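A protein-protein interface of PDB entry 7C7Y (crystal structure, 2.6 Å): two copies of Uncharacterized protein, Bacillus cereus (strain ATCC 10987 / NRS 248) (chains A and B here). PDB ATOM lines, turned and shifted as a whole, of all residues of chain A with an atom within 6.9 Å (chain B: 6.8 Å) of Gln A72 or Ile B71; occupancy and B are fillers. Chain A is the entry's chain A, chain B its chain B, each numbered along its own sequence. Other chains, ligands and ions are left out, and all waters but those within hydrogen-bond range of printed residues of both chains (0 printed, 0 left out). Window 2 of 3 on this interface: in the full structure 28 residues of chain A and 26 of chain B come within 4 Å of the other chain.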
ATOM      1  N   MET A  65      -3.577  15.348  15.737  1.00  0.00           N
ATOM      2  CA  MET A  65      -2.583  14.424  15.145  1.00  0.00           C
ATOM      3  C   MET A  65      -1.732  13.856  16.275  1.00  0.00           C
ATOM      4  O   MET A  65      -1.508  12.676  16.247  1.00  0.00           O
ATOM      5  CB  MET A  65      -1.668  15.098  14.116  1.00  0.00           C
ATOM      6  CG  MET A  65      -2.005  14.833  12.665  1.00  0.00           C
ATOM      7  SD  MET A  65      -2.371  12.958  12.175  1.00  0.00           S
ATOM      8  CE  MET A  65      -1.186  11.883  13.309  1.00  0.00           C
ATOM      9  N   THR A  67      -2.597  13.210  19.197  1.00  0.00           N
ATOM     10  CA  THR A  67      -3.455  12.192  19.854  1.00  0.00           C
ATOM     11  C   THR A  67      -3.542  10.930  18.988  1.00  0.00           C
ATOM     12  O   THR A  67      -3.275   9.834  19.511  1.00  0.00           O
ATOM     13  CB  THR A  67      -4.845  12.743  20.178  1.00  0.00           C
ATOM     14  OG1 THR A  67      -4.656  13.762  21.157  1.00  0.00           O
ATOM     15  CG2 THR A  67      -5.773  11.668  20.695  1.00  0.00           C
ATOM     16  N   ILE A  68      -3.909  11.071  17.715  1.00  0.00           N
ATOM     17  CA  ILE A  68      -4.109   9.914  16.800  1.00  0.00           C
ATOM     18  C   ILE A  68      -2.755   9.234  16.591  1.00  0.00           C
ATOM     19  O   ILE A  68      -2.745   8.094  16.157  1.00  0.00           O
ATOM     20  CB  ILE A  68      -4.789  10.370  15.492  1.00  0.00           C
ATOM     21  CG1 ILE A  68      -6.246  10.755  15.749  1.00  0.00           C
ATOM     22  CG2 ILE A  68      -4.682   9.323  14.402  1.00  0.00           C
ATOM     23  CD1 ILE A  68      -6.862  11.606  14.662  1.00  0.00           C
ATOM     24  N   ARG A  69      -1.655   9.907  16.924  1.00  0.00           N
ATOM     25  CA  ARG A  69      -0.272   9.362  16.820  1.00  0.00           C
ATOM     26  C   ARG A  69       0.035   8.506  18.056  1.00  0.00           C
ATOM     27  O   ARG A  69       0.661   7.457  17.895  1.00  0.00           O
ATOM     28  CB  ARG A  69       0.729  10.509  16.646  1.00  0.00           C
ATOM     29  CG  ARG A  69       2.184  10.074  16.546  1.00  0.00           C
ATOM     30  CD  ARG A  69       2.488   9.356  15.240  1.00  0.00           C
ATOM     31  NE  ARG A  69       3.828   8.767  15.252  1.00  0.00           N
ATOM     32  CZ  ARG A  69       4.109   7.462  15.272  1.00  0.00           C
ATOM     33  NH1 ARG A  69       3.150   6.551  15.267  1.00  0.00           N
ATOM     34  NH2 ARG A  69       5.368   7.069  15.281  1.00  0.00           N
ATOM     35  N   LEU A  70      -0.372   8.953  19.245  1.00  0.00           N
ATOM     36  CA  LEU A  70      -0.247   8.192  20.522  1.00  0.00           C
ATOM     37  C   LEU A  70      -1.164   6.956  20.520  1.00  0.00           C
ATOM     38  O   LEU A  70      -0.647   5.841  20.821  1.00  0.00           O
ATOM     39  CB  LEU A  70      -0.573   9.107  21.709  1.00  0.00           C
ATOM     40  CG  LEU A  70       0.616   9.535  22.569  1.00  0.00           C
ATOM     41  CD1 LEU A  70       1.768  10.052  21.709  1.00  0.00           C
ATOM     42  CD2 LEU A  70       0.182  10.594  23.567  1.00  0.00           C
ATOM     43  N   ILE A  71      -2.464   7.125  20.217  1.00  0.00           N
ATOM     44  CA  ILE A  71      -3.435   5.986  20.149  1.00  0.00           C
ATOM     45  C   ILE A  71      -2.782   4.865  19.337  1.00  0.00           C
ATOM     46  O   ILE A  71      -2.912   3.692  19.715  1.00  0.00           O
ATOM     47  CB  ILE A  71      -4.783   6.380  19.516  1.00  0.00           C
ATOM     48  CG1 ILE A  71      -5.428   7.602  20.177  1.00  0.00           C
ATOM     49  CG2 ILE A  71      -5.725   5.188  19.505  1.00  0.00           C
ATOM     50  CD1 ILE A  71      -5.480   7.562  21.681  1.00  0.00           C
ATOM     51  N   GLN A  72      -2.095   5.243  18.266  1.00  0.00           N
ATOM     52  CA  GLN A  72      -1.363   4.327  17.365  1.00  0.00           C
ATOM     53  C   GLN A  72      -0.202   3.663  18.105  1.00  0.00           C
ATOM     54  O   GLN A  72      -0.036   2.443  17.945  1.00  0.00           O
ATOM     55  CB  GLN A  72      -0.810   5.100  16.174  1.00  0.00           C
ATOM     56  CG  GLN A  72      -1.230   4.508  14.845  1.00  0.00           C
ATOM     57  CD  GLN A  72      -0.416   5.070  13.713  1.00  0.00           C
ATOM     58  OE1 GLN A  72      -0.513   4.602  12.582  1.00  0.00           O
ATOM     59  NE2 GLN A  72       0.393   6.074  14.015  1.00  0.00           N
ATOM     60  N   GLU A  73       0.596   4.434  18.843  1.00  0.00           N
ATOM     61  CA  GLU A  73       1.699   3.891  19.680  1.00  0.00           C
ATOM     62  C   GLU A  73       1.111   3.346  20.986  1.00  0.00           C
ATOM     63  O   GLU A  73       1.367   2.198  21.308  1.00  0.00           O
ATOM     64  CB  GLU A  73       2.747   4.969  19.942  1.00  0.00           C
ATOM     65  CG  GLU A  73       3.354   5.513  18.665  1.00  0.00           C
ATOM     66  CD  GLU A  73       4.646   6.284  18.863  1.00  0.00           C
ATOM     67  OE1 GLU A  73       4.612   7.305  19.584  1.00  0.00           O
ATOM     68  OE2 GLU A  73       5.686   5.855  18.304  1.00  0.00           O
ATOM     69  N   SER B  66     -10.730  11.715   7.010  1.00  0.00           N
ATOM     70  CA  SER B  66      -9.848  10.895   6.144  1.00  0.00           C
ATOM     71  C   SER B  66      -8.743  10.314   7.008  1.00  0.00           C
ATOM     72  O   SER B  66      -8.488   9.110   6.897  1.00  0.00           O
ATOM     73  CB  SER B  66      -9.280  11.689   4.991  1.00  0.00           C
ATOM     74  OG  SER B  66      -8.269  10.967   4.283  1.00  0.00           O
ATOM     75  N   THR B  67      -8.132  11.131   7.857  1.00  0.00           N
ATOM     76  CA  THR B  67      -7.076  10.656   8.779  1.00  0.00           C
ATOM     77  C   THR B  67      -7.596   9.455   9.566  1.00  0.00           C
ATOM     78  O   THR B  67      -7.068   8.362   9.358  1.00  0.00           O
ATOM     79  CB  THR B  67      -6.598  11.738   9.746  1.00  0.00           C
ATOM     80  OG1 THR B  67      -6.172  12.838   8.956  1.00  0.00           O
ATOM     81  CG2 THR B  67      -5.443  11.274  10.599  1.00  0.00           C
ATOM     82  N   ILE B  68      -8.615   9.651  10.407  1.00  0.00           N
ATOM     83  CA  ILE B  68      -9.142   8.596  11.325  1.00  0.00           C
ATOM     84  C   ILE B  68      -9.375   7.318  10.518  1.00  0.00           C
ATOM     85  O   ILE B  68      -8.816   6.314  10.896  1.00  0.00           O
ATOM     86  CB  ILE B  68     -10.395   9.081  12.092  1.00  0.00           C
ATOM     87  CG1 ILE B  68     -10.015  10.131  13.141  1.00  0.00           C
ATOM     88  CG2 ILE B  68     -11.165   7.918  12.711  1.00  0.00           C
ATOM     89  CD1 ILE B  68     -10.964  10.208  14.295  1.00  0.00           C
ATOM     90  N   ARG B  69     -10.118   7.367   9.416  1.00  0.00           N
ATOM     91  CA  ARG B  69     -10.398   6.178   8.560  1.00  0.00           C
ATOM     92  C   ARG B  69      -9.089   5.555   8.034  1.00  0.00           C
ATOM     93  O   ARG B  69      -8.958   4.329   8.170  1.00  0.00           O
ATOM     94  CB  ARG B  69     -11.354   6.549   7.421  1.00  0.00           C
ATOM     95  CG  ARG B  69     -12.761   6.911   7.884  1.00  0.00           C
ATOM     96  CD  ARG B  69     -13.755   6.881   6.738  1.00  0.00           C
ATOM     97  NE  ARG B  69     -13.862   5.537   6.178  1.00  0.00           N
ATOM     98  CZ  ARG B  69     -14.262   5.233   4.940  1.00  0.00           C
ATOM     99  NH1 ARG B  69     -14.608   6.182   4.085  1.00  0.00           N
ATOM    100  NH2 ARG B  69     -14.308   3.967   4.553  1.00  0.00           N
ATOM    101  N   LEU B  70      -8.157   6.341   7.470  1.00  0.00           N
ATOM    102  CA  LEU B  70      -6.853   5.849   6.936  1.00  0.00           C
ATOM    103  C   LEU B  70      -6.012   5.217   8.046  1.00  0.00           C
ATOM    104  O   LEU B  70      -5.389   4.155   7.804  1.00  0.00           O
ATOM    105  CB  LEU B  70      -6.049   7.008   6.335  1.00  0.00           C
ATOM    106  CG  LEU B  70      -6.122   7.175   4.817  1.00  0.00           C
ATOM    107  CD1 LEU B  70      -5.221   8.319   4.385  1.00  0.00           C
ATOM    108  CD2 LEU B  70      -5.755   5.887   4.083  1.00  0.00           C
ATOM    109  N   ILE B  71      -5.938   5.880   9.201  1.00  0.00           N
ATOM    110  CA  ILE B  71      -5.017   5.495  10.302  1.00  0.00           C
ATOM    111  C   ILE B  71      -5.585   4.291  11.051  1.00  0.00           C
ATOM    112  O   ILE B  71      -4.790   3.423  11.355  1.00  0.00           O
ATOM    113  CB  ILE B  71      -4.744   6.677  11.249  1.00  0.00           C
ATOM    114  CG1 ILE B  71      -4.159   7.889  10.522  1.00  0.00           C
ATOM    115  CG2 ILE B  71      -3.854   6.236  12.392  1.00  0.00           C
ATOM    116  CD1 ILE B  71      -2.955   7.575   9.648  1.00  0.00           C
ATOM    117  N   GLN B  72      -6.896   4.252  11.339  1.00  0.00           N
ATOM    118  CA  GLN B  72      -7.512   3.341  12.354  1.00  0.00           C
ATOM    119  C   GLN B  72      -8.493   2.334  11.739  1.00  0.00           C
ATOM    120  O   GLN B  72      -8.784   1.346  12.412  1.00  0.00           O
ATOM    121  CB  GLN B  72      -8.238   4.150  13.431  1.00  0.00           C
ATOM    122  CG  GLN B  72      -7.350   5.177  14.128  1.00  0.00           C
ATOM    123  CD  GLN B  72      -8.102   5.928  15.202  1.00  0.00           C
ATOM    124  OE1 GLN B  72      -9.326   6.050  15.160  1.00  0.00           O
ATOM    125  NE2 GLN B  72      -7.374   6.447  16.178  1.00  0.00           N
ATOM    126  N   GLU B  73      -9.000   2.563  10.528  1.00  0.00           N
ATOM    127  CA  GLU B  73      -9.983   1.656   9.874  1.00  0.00           C
ATOM    128  C   GLU B  73      -9.260   0.726   8.896  1.00  0.00           C
ATOM    129  O   GLU B  73      -9.790  -0.335   8.555  1.00  0.00           O
ATOM    130  CB  GLU B  73     -11.046   2.486   9.160  1.00  0.00           C
ATOM    131  CG  GLU B  73     -12.281   1.707   8.774  1.00  0.00           C
ATOM    132  CD  GLU B  73     -13.235   2.517   7.914  1.00  0.00           C
ATOM    133  OE1 GLU B  73     -13.336   3.731   8.154  1.00  0.00           O
ATOM    134  OE2 GLU B  73     -13.855   1.944   6.996  1.00  0.00           O
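NE2 of Gln A72 sits close to NH1 of Arg A69 (3.1 Å).
Among the printed residues, merely in contact across the chains: Met A65 with Thr B67 (3.8 Å), Ile A68 with Ile B68 (3.8 Å), Ile A68 with Ile B71 (3.8 Å), Ile A71 with Gln B72 (3.9 Å) and Gln A72 with Ile B71 (3.7 Å).
Of chain B, only Ile B71 comes within 4 Å of Gln A72.
Printed residues of chain A within 4 Å of Ile B71: Ile A68 (3.8 Å) and Gln A72 (3.7 Å).
Of the printed residues of chain A, Ile B68 touches Ile A68.
Of the printed residues of chain B, Ile A71 touches Gln B72.
The nearest printed residue of chain A that does not touch Gln B72 is Ile A68 (4.3 Å).
Hydrophobic or aromatic side chains of chain A that line the printed part of chain B: Met A65, Ile A68 and Ile A71.
Hydrophobic or aromatic side chains of chain B within 4 Å of the printed part of chain A: Ile B68 and Ile B71.
Among the printed residues, 5 pairs touch across the chains.
Among the printed residues, no Asp or Glu carboxylate lies within 4 Å of a Lys or Arg side-chain nitrogen of the other chain.
Ile A68 touches its own counterpart, Ile B68.
Ile A68 touches Ile B71, but with the chains exchanged Ile A71 does not touch Ile B68 (8.5 Å).
Ile A71 touches Gln B72, and with the chains exchanged Gln A72 touches Ile B71.
7 positions are printed for both chains.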
